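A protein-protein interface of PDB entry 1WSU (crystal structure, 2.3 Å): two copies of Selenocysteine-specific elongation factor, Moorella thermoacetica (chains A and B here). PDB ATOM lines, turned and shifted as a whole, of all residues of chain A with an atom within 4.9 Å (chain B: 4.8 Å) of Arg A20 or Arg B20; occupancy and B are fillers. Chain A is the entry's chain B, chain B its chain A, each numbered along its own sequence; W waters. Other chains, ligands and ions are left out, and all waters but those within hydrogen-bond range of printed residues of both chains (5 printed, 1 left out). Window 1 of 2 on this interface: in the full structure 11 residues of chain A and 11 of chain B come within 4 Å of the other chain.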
ATOM      1  N   TYR A  16       6.240 -28.129  19.725  1.00  0.00           N
ATOM      2  CA  TYR A  16       5.518 -28.206  20.987  1.00  0.00           C
ATOM      3  C   TYR A  16       5.160 -26.827  21.534  1.00  0.00           C
ATOM      4  O   TYR A  16       4.148 -26.669  22.193  1.00  0.00           O
ATOM      5  CB  TYR A  16       6.308 -28.994  22.021  1.00  0.00           C
ATOM      6  CG  TYR A  16       6.229 -30.483  21.795  1.00  0.00           C
ATOM      7  CD1 TYR A  16       7.122 -31.129  20.927  1.00  0.00           C
ATOM      8  CD2 TYR A  16       5.214 -31.248  22.399  1.00  0.00           C
ATOM      9  CE1 TYR A  16       7.008 -32.503  20.660  1.00  0.00           C
ATOM     10  CE2 TYR A  16       5.088 -32.616  22.133  1.00  0.00           C
ATOM     11  CZ  TYR A  16       5.987 -33.231  21.264  1.00  0.00           C
ATOM     12  OH  TYR A  16       5.846 -34.560  20.984  1.00  0.00           O
ATOM     13  N   ARG A  17       5.983 -25.833  21.230  1.00  0.00           N
ATOM     14  CA  ARG A  17       5.757 -24.475  21.693  1.00  0.00           C
ATOM     15  C   ARG A  17       4.547 -23.889  20.994  1.00  0.00           C
ATOM     16  O   ARG A  17       3.658 -23.316  21.621  1.00  0.00           O
ATOM     17  CB  ARG A  17       7.000 -23.631  21.404  1.00  0.00           C
ATOM     18  CG  ARG A  17       6.766 -22.142  21.374  1.00  0.00           C
ATOM     19  CD  ARG A  17       7.826 -21.423  22.166  1.00  0.00           C
ATOM     20  NE  ARG A  17       9.157 -21.937  21.892  1.00  0.00           N
ATOM     21  CZ  ARG A  17      10.160 -21.886  22.764  1.00  0.00           C
ATOM     22  NH1 ARG A  17      11.346 -22.376  22.438  1.00  0.00           N
ATOM     23  NH2 ARG A  17       9.977 -21.356  23.966  1.00  0.00           N
ATOM     24  N   VAL A  18       4.515 -24.040  19.683  1.00  0.00           N
ATOM     25  CA  VAL A  18       3.414 -23.533  18.897  1.00  0.00           C
ATOM     26  C   VAL A  18       2.108 -24.232  19.279  1.00  0.00           C
ATOM     27  O   VAL A  18       1.125 -23.568  19.582  1.00  0.00           O
ATOM     28  CB  VAL A  18       3.743 -23.680  17.396  1.00  0.00           C
ATOM     29  CG1 VAL A  18       2.560 -23.276  16.513  1.00  0.00           C
ATOM     30  CG2 VAL A  18       4.940 -22.792  17.082  1.00  0.00           C
ATOM     31  N   SER A  19       2.104 -25.559  19.306  1.00  0.00           N
ATOM     32  CA  SER A  19       0.896 -26.317  19.648  1.00  0.00           C
ATOM     33  C   SER A  19       0.402 -26.119  21.082  1.00  0.00           C
ATOM     34  O   SER A  19      -0.767 -26.361  21.368  1.00  0.00           O
ATOM     35  CB  SER A  19       1.121 -27.806  19.390  1.00  0.00           C
ATOM     36  OG  SER A  19       1.523 -28.005  18.051  1.00  0.00           O
ATOM     37  N   ARG A  20       1.296 -25.702  21.977  1.00  0.00           N
ATOM     38  CA  ARG A  20       0.950 -25.415  23.361  1.00  0.00           C
ATOM     39  C   ARG A  20       0.076 -26.379  24.132  1.00  0.00           C
ATOM     40  O   ARG A  20       0.566 -27.355  24.676  1.00  0.00           O
ATOM     41  CB  ARG A  20       0.296 -24.022  23.503  1.00  0.00           C
ATOM     42  CG  ARG A  20       1.209 -22.970  24.095  1.00  0.00           C
ATOM     43  CD  ARG A  20       0.591 -22.084  25.210  1.00  0.00           C
ATOM     44  NE  ARG A  20      -0.713 -21.525  24.890  1.00  0.00           N
ATOM     45  CZ  ARG A  20      -1.239 -20.435  25.458  1.00  0.00           C
ATOM     46  NH1 ARG A  20      -0.585 -19.732  26.391  1.00  0.00           N
ATOM     47  NH2 ARG A  20      -2.452 -20.054  25.098  1.00  0.00           N
ATOM     48  N   TRP A  21      -1.217 -26.059  24.210  1.00  0.00           N
ATOM     49  CA  TRP A  21      -2.173 -26.835  24.993  1.00  0.00           C
ATOM     50  C   TRP A  21      -2.897 -27.917  24.240  1.00  0.00           C
ATOM     51  O   TRP A  21      -3.769 -28.587  24.786  1.00  0.00           O
ATOM     52  CB  TRP A  21      -3.173 -25.894  25.670  1.00  0.00           C
ATOM     53  CG  TRP A  21      -2.498 -24.903  26.558  1.00  0.00           C
ATOM     54  CD1 TRP A  21      -1.250 -25.017  27.119  1.00  0.00           C
ATOM     55  CD2 TRP A  21      -3.039 -23.663  27.032  1.00  0.00           C
ATOM     56  NE1 TRP A  21      -0.987 -23.920  27.913  1.00  0.00           N
ATOM     57  CE2 TRP A  21      -2.072 -23.077  27.875  1.00  0.00           C
ATOM     58  CE3 TRP A  21      -4.251 -22.996  26.834  1.00  0.00           C
ATOM     59  CZ2 TRP A  21      -2.283 -21.857  28.517  1.00  0.00           C
ATOM     60  CZ3 TRP A  21      -4.458 -21.783  27.471  1.00  0.00           C
ATOM     61  CH2 TRP A  21      -3.478 -21.226  28.303  1.00  0.00           C
ATOM     62  N   GLN A  22      -2.533 -28.072  22.978  1.00  0.00           N
ATOM     63  CA  GLN A  22      -3.083 -29.122  22.129  1.00  0.00           C
ATOM     64  C   GLN A  22      -1.850 -29.680  21.406  1.00  0.00           C
ATOM     65  O   GLN A  22      -1.734 -29.620  20.182  1.00  0.00           O
ATOM     66  CB  GLN A  22      -4.086 -28.546  21.132  1.00  0.00           C
ATOM     67  CG  GLN A  22      -5.319 -27.926  21.783  1.00  0.00           C
ATOM     68  CD  GLN A  22      -5.089 -26.492  22.245  1.00  0.00           C
ATOM     69  OE1 GLN A  22      -4.621 -25.652  21.476  1.00  0.00           O
ATOM     70  NE2 GLN A  22      -5.433 -26.203  23.497  1.00  0.00           N
ATOM     71  N   PRO A  23      -0.897 -30.208  22.185  1.00  0.00           N
ATOM     72  CA  PRO A  23       0.354 -30.774  21.673  1.00  0.00           C
ATOM     73  C   PRO A  23       0.073 -31.944  20.762  1.00  0.00           C
ATOM     74  O   PRO A  23      -0.936 -32.614  20.922  1.00  0.00           O
ATOM     75  CB  PRO A  23       1.090 -31.185  22.945  1.00  0.00           C
ATOM     76  CG  PRO A  23      -0.049 -31.608  23.857  1.00  0.00           C
ATOM     77  CD  PRO A  23      -1.075 -30.522  23.617  1.00  0.00           C
ATOM     78  N   TRP A  62       4.455 -32.067  26.696  1.00  0.00           N
ATOM     79  CA  TRP A  62       4.079 -30.660  26.666  1.00  0.00           C
ATOM     80  C   TRP A  62       5.346 -29.820  26.699  1.00  0.00           C
ATOM     81  O   TRP A  62       6.356 -30.204  27.299  1.00  0.00           O
ATOM     82  CB  TRP A  62       3.207 -30.267  27.895  1.00  0.00           C
ATOM     83  CG  TRP A  62       1.725 -30.594  27.772  1.00  0.00           C
ATOM     84  CD1 TRP A  62       1.178 -31.766  27.330  1.00  0.00           C
ATOM     85  CD2 TRP A  62       0.618 -29.736  28.096  1.00  0.00           C
ATOM     86  NE1 TRP A  62      -0.194 -31.690  27.357  1.00  0.00           N
ATOM     87  CE2 TRP A  62      -0.563 -30.456  27.819  1.00  0.00           C
ATOM     88  CE3 TRP A  62       0.510 -28.429  28.590  1.00  0.00           C
ATOM     89  CZ2 TRP A  62      -1.841 -29.911  28.018  1.00  0.00           C
ATOM     90  CZ3 TRP A  62      -0.764 -27.886  28.790  1.00  0.00           C
ATOM     91  CH2 TRP A  62      -1.924 -28.632  28.501  1.00  0.00           C
ATOM     92  N   ALA A  66       4.527 -24.105  28.125  1.00  0.00           N
ATOM     93  CA  ALA A  66       3.094 -24.221  27.928  1.00  0.00           C
ATOM     94  C   ALA A  66       2.454 -24.863  29.151  1.00  0.00           C
ATOM     95  O   ALA A  66       1.290 -24.611  29.452  1.00  0.00           O
ATOM     96  CB  ALA A  66       2.799 -25.048  26.714  1.00  0.00           C
ATOM     97  N   GLU A  69       2.232 -22.185  31.931  1.00  0.00           N
ATOM     98  CA  GLU A  69       1.144 -21.260  31.714  1.00  0.00           C
ATOM     99  C   GLU A  69      -0.192 -21.908  31.985  1.00  0.00           C
ATOM    100  O   GLU A  69      -1.097 -21.256  32.478  1.00  0.00           O
ATOM    101  CB  GLU A  69       1.155 -20.717  30.280  1.00  0.00           C
ATOM    102  CG  GLU A  69       2.299 -19.790  29.970  1.00  0.00           C
ATOM    103  CD  GLU A  69       1.825 -18.606  29.139  1.00  0.00           C
ATOM    104  OE1 GLU A  69       1.530 -17.548  29.744  1.00  0.00           O
ATOM    105  OE2 GLU A  69       1.723 -18.740  27.890  1.00  0.00           O
ATOM    106  N   TYR B  16      -5.639 -12.520  28.087  1.00  0.00           N
ATOM    107  CA  TYR B  16      -4.485 -12.365  27.216  1.00  0.00           C
ATOM    108  C   TYR B  16      -3.592 -13.600  27.211  1.00  0.00           C
ATOM    109  O   TYR B  16      -3.064 -13.969  26.184  1.00  0.00           O
ATOM    110  CB  TYR B  16      -3.683 -11.119  27.611  1.00  0.00           C
ATOM    111  CG  TYR B  16      -4.332  -9.811  27.202  1.00  0.00           C
ATOM    112  CD1 TYR B  16      -5.182  -9.104  28.074  1.00  0.00           C
ATOM    113  CD2 TYR B  16      -4.097  -9.275  25.932  1.00  0.00           C
ATOM    114  CE1 TYR B  16      -5.776  -7.892  27.679  1.00  0.00           C
ATOM    115  CE2 TYR B  16      -4.686  -8.076  25.528  1.00  0.00           C
ATOM    116  CZ  TYR B  16      -5.521  -7.395  26.397  1.00  0.00           C
ATOM    117  OH  TYR B  16      -6.118  -6.246  25.939  1.00  0.00           O
ATOM    118  N   ARG B  17      -3.432 -14.239  28.360  1.00  0.00           N
ATOM    119  CA  ARG B  17      -2.613 -15.436  28.453  1.00  0.00           C
ATOM    120  C   ARG B  17      -3.210 -16.537  27.553  1.00  0.00           C
ATOM    121  O   ARG B  17      -2.510 -17.178  26.775  1.00  0.00           O
ATOM    122  CB  ARG B  17      -2.550 -15.872  29.923  1.00  0.00           C
ATOM    123  CG  ARG B  17      -2.287 -17.352  30.174  1.00  0.00           C
ATOM    124  CD  ARG B  17      -1.036 -17.580  31.011  1.00  0.00           C
ATOM    125  NE  ARG B  17      -0.972 -16.820  32.263  1.00  0.00           N
ATOM    126  CZ  ARG B  17       0.176 -16.409  32.807  1.00  0.00           C
ATOM    127  NH1 ARG B  17       0.183 -15.731  33.936  1.00  0.00           N
ATOM    128  NH2 ARG B  17       1.334 -16.664  32.213  1.00  0.00           N
ATOM    129  N   VAL B  18      -4.514 -16.736  27.648  1.00  0.00           N
ATOM    130  CA  VAL B  18      -5.182 -17.740  26.844  1.00  0.00           C
ATOM    131  C   VAL B  18      -5.147 -17.381  25.369  1.00  0.00           C
ATOM    132  O   VAL B  18      -4.689 -18.179  24.557  1.00  0.00           O
ATOM    133  CB  VAL B  18      -6.636 -17.936  27.331  1.00  0.00           C
ATOM    134  CG1 VAL B  18      -7.420 -18.844  26.374  1.00  0.00           C
ATOM    135  CG2 VAL B  18      -6.612 -18.551  28.744  1.00  0.00           C
ATOM    136  N   SER B  19      -5.604 -16.181  25.022  1.00  0.00           N
ATOM    137  CA  SER B  19      -5.620 -15.723  23.622  1.00  0.00           C
ATOM    138  C   SER B  19      -4.237 -15.765  22.970  1.00  0.00           C
ATOM    139  O   SER B  19      -4.111 -15.914  21.758  1.00  0.00           O
ATOM    140  CB  SER B  19      -6.187 -14.314  23.544  1.00  0.00           C
ATOM    141  OG  SER B  19      -7.579 -14.338  23.786  1.00  0.00           O
ATOM    142  N   ARG B  20      -3.208 -15.598  23.794  1.00  0.00           N
ATOM    143  CA  ARG B  20      -1.823 -15.699  23.382  1.00  0.00           C
ATOM    144  C   ARG B  20      -1.337 -14.898  22.174  1.00  0.00           C
ATOM    145  O   ARG B  20      -1.095 -13.703  22.293  1.00  0.00           O
ATOM    146  CB  ARG B  20      -1.501 -17.176  23.165  1.00  0.00           C
ATOM    147  CG  ARG B  20      -0.059 -17.525  23.412  1.00  0.00           C
ATOM    148  CD  ARG B  20       0.279 -18.859  22.791  1.00  0.00           C
ATOM    149  NE  ARG B  20       1.539 -19.356  23.318  1.00  0.00           N
ATOM    150  CZ  ARG B  20       2.214 -20.355  22.774  1.00  0.00           C
ATOM    151  NH1 ARG B  20       1.735 -20.941  21.691  1.00  0.00           N
ATOM    152  NH2 ARG B  20       3.340 -20.782  23.337  1.00  0.00           N
ATOM    153  N   TRP B  21      -1.160 -15.566  21.028  1.00  0.00           N
ATOM    154  CA  TRP B  21      -0.677 -14.914  19.808  1.00  0.00           C
ATOM    155  C   TRP B  21      -1.771 -14.302  18.954  1.00  0.00           C
ATOM    156  O   TRP B  21      -1.494 -13.736  17.898  1.00  0.00           O
ATOM    157  CB  TRP B  21       0.171 -15.870  18.962  1.00  0.00           C
ATOM    158  CG  TRP B  21       1.397 -16.304  19.687  1.00  0.00           C
ATOM    159  CD1 TRP B  21       1.964 -15.681  20.765  1.00  0.00           C
ATOM    160  CD2 TRP B  21       2.185 -17.481  19.438  1.00  0.00           C
ATOM    161  NE1 TRP B  21       3.052 -16.403  21.213  1.00  0.00           N
ATOM    162  CE2 TRP B  21       3.207 -17.513  20.416  1.00  0.00           C
ATOM    163  CE3 TRP B  21       2.125 -18.512  18.490  1.00  0.00           C
ATOM    164  CZ2 TRP B  21       4.164 -18.547  20.477  1.00  0.00           C
ATOM    165  CZ3 TRP B  21       3.083 -19.554  18.551  1.00  0.00           C
ATOM    166  CH2 TRP B  21       4.082 -19.554  19.542  1.00  0.00           C
ATOM    167  N   GLN B  22      -3.014 -14.428  19.402  1.00  0.00           N
ATOM    168  CA  GLN B  22      -4.140 -13.785  18.720  1.00  0.00           C
ATOM    169  C   GLN B  22      -4.920 -13.016  19.799  1.00  0.00           C
ATOM    170  O   GLN B  22      -6.129 -13.194  19.961  1.00  0.00           O
ATOM    171  CB  GLN B  22      -5.046 -14.807  18.056  1.00  0.00           C
ATOM    172  CG  GLN B  22      -4.405 -15.528  16.870  1.00  0.00           C
ATOM    173  CD  GLN B  22      -3.568 -16.727  17.282  1.00  0.00           C
ATOM    174  OE1 GLN B  22      -4.070 -17.656  17.922  1.00  0.00           O
ATOM    175  NE2 GLN B  22      -2.290 -16.717  16.912  1.00  0.00           N
ATOM    176  N   PRO B  23      -4.223 -12.149  20.556  1.00  0.00           N
ATOM    177  CA  PRO B  23      -4.805 -11.341  21.637  1.00  0.00           C
ATOM    178  C   PRO B  23      -6.011 -10.550  21.193  1.00  0.00           C
ATOM    179  O   PRO B  23      -6.076 -10.136  20.048  1.00  0.00           O
ATOM    180  CB  PRO B  23      -3.666 -10.405  22.025  1.00  0.00           C
ATOM    181  CG  PRO B  23      -3.008 -10.158  20.716  1.00  0.00           C
ATOM    182  CD  PRO B  23      -2.929 -11.584  20.144  1.00  0.00           C
ATOM    183  N   TRP B  62      -0.133  -7.541  24.373  1.00  0.00           N
ATOM    184  CA  TRP B  62       0.214  -8.960  24.365  1.00  0.00           C
ATOM    185  C   TRP B  62       0.640  -9.357  25.783  1.00  0.00           C
ATOM    186  O   TRP B  62       1.239  -8.556  26.524  1.00  0.00           O
ATOM    187  CB  TRP B  62       1.403  -9.243  23.420  1.00  0.00           C
ATOM    188  CG  TRP B  62       1.071  -9.407  21.959  1.00  0.00           C
ATOM    189  CD1 TRP B  62       0.207  -8.653  21.226  1.00  0.00           C
ATOM    190  CD2 TRP B  62       1.572 -10.422  21.068  1.00  0.00           C
ATOM    191  NE1 TRP B  62       0.127  -9.138  19.938  1.00  0.00           N
ATOM    192  CE2 TRP B  62       0.954 -10.221  19.814  1.00  0.00           C
ATOM    193  CE3 TRP B  62       2.477 -11.480  21.209  1.00  0.00           C
ATOM    194  CZ2 TRP B  62       1.212 -11.042  18.707  1.00  0.00           C
ATOM    195  CZ3 TRP B  62       2.736 -12.298  20.102  1.00  0.00           C
ATOM    196  CH2 TRP B  62       2.101 -12.071  18.870  1.00  0.00           C
ATOM    197  N   ALA B  66       3.433 -14.560  26.271  1.00  0.00           N
ATOM    198  CA  ALA B  66       3.110 -14.847  24.874  1.00  0.00           C
ATOM    199  C   ALA B  66       4.179 -14.243  23.967  1.00  0.00           C
ATOM    200  O   ALA B  66       4.647 -14.891  23.038  1.00  0.00           O
ATOM    201  CB  ALA B  66       1.773 -14.257  24.517  1.00  0.00           C
ATOM    202  N   GLU B  69       7.556 -16.000  24.077  1.00  0.00           N
ATOM    203  CA  GLU B  69       7.544 -17.240  23.328  1.00  0.00           C
ATOM    204  C   GLU B  69       7.578 -16.957  21.850  1.00  0.00           C
ATOM    205  O   GLU B  69       8.231 -17.667  21.098  1.00  0.00           O
ATOM    206  CB  GLU B  69       6.298 -18.059  23.664  1.00  0.00           C
ATOM    207  CG  GLU B  69       6.326 -18.563  25.070  1.00  0.00           C
ATOM    208  CD  GLU B  69       6.593 -20.036  25.115  1.00  0.00           C
ATOM    209  OE1 GLU B  69       5.605 -20.802  25.228  1.00  0.00           O
ATOM    210  OE2 GLU B  69       7.785 -20.425  25.017  1.00  0.00           O
HETATM  211  O   HOH W   1       0.860 -16.318  27.295  1.00  0.00           O
HETATM  212  O   HOH W   2       2.789 -18.172  25.198  1.00  0.00           O
HETATM  213  O   HOH W   3       3.470 -17.914  31.639  1.00  0.00           O
HETATM  214  O   HOH W   4      -0.633 -20.588  19.865  1.00  0.00           O
HETATM  215  O   HOH W   5       4.902 -23.135  24.963  1.00  0.00           O
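Printed residues of chain A that touch a printed residue of chain B: Arg A17, Val A18, Arg A20 and Glu A69.
Printed residues of chain B that touch a printed residue of chain A: Arg B17, Val B18, Arg B20 and Glu B69.
Among the printed residues, 7 pairs touch across the chains.
NH2 of Arg B20 is in salt-bridge range of OE1 of Glu B69 (3.0 Å).
The guanidinium group (NH1) of Arg A20 is in salt-bridge range of the side-chain carboxylate (OE2) of Glu A69 (2.9 Å).
Printed residues of chain B within 4 Å of Arg A17: Arg B20 (3.1 Å) and Glu B69 (2.6 Å).
Printed residues of chain B within 4 Å of Val A18: Arg B20 (3.4 Å).
Of the printed residues of chain A, Arg B17 touches Arg A20 (3.2 Å) and Glu A69 (2.6 Å).
Of the printed residues of chain A, Val B18 touches Arg A20.
Of the printed residues of chain A, Arg B20 touches Arg A17 (3.1 Å), Val A18 (3.4 Å) and Arg A20 (3.1 Å).
Of the printed residues of chain A, Glu B69 touches Arg A17.
Arg A17 touches Arg B20, and with the chains exchanged Arg A20 touches Arg B17.
Arg A17 touches Glu B69, and with the chains exchanged Glu A69 touches Arg B17.
Val A18 touches Arg B20, and with the chains exchanged Arg A20 touches Val B18.
Arg A20 touches its own counterpart, Arg B20.
11 positions are printed for both chains.
Water W5 lies within hydrogen-bond range of OE1 of Glu B69, NH2 of Arg B20 and N of Ala A66.
Water W3 lies within hydrogen-bond range of NH2 of Arg B17 (2.5 Å) and OE1 of Glu A69 (2.7 Å).
Water W2 lies within hydrogen-bond range of the guanidinium group of Arg B20 and the side-chain carboxylate of Glu A69.
Water W1 bridges the side-chain carboxylate (OE2) of Glu A69 (2.6 Å) and the backbone NH (N) of Ala B66 (3.3 Å).
Water W4 bridges NH1 of Arg B20 (3.0 Å) and O of Val A18 (3.5 Å).
O of Arg B17 sits at hydrogen-bond distance from NH1 of Arg A20 (3.2 Å).
The guanidinium group (NH2) of Arg B17 lies within salt-bridge range of the side-chain carboxylate (OE1) of Glu A69, at 2.6 Å.
The backbone carbonyl oxygen of Val B18 lies within hydrogen-bond range of the guanidinium group of Arg A20 (3.0 Å).
NH1 of Arg B20 sits at hydrogen-bond distance from O of Arg A17, at 3.1 Å.
The guanidinium group of Arg B20 lies within hydrogen-bond range of the backbone carbonyl oxygen of Val A18, at 3.4 Å.
The side-chain carboxylate of Glu B69 lies within salt-bridge range of the guanidinium group of Arg A17 (2.6 Å).
The guanidinium group (NE) of Arg A20 sits close to the guanidinium group (NE) of Arg B20, at 3.5 Å.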
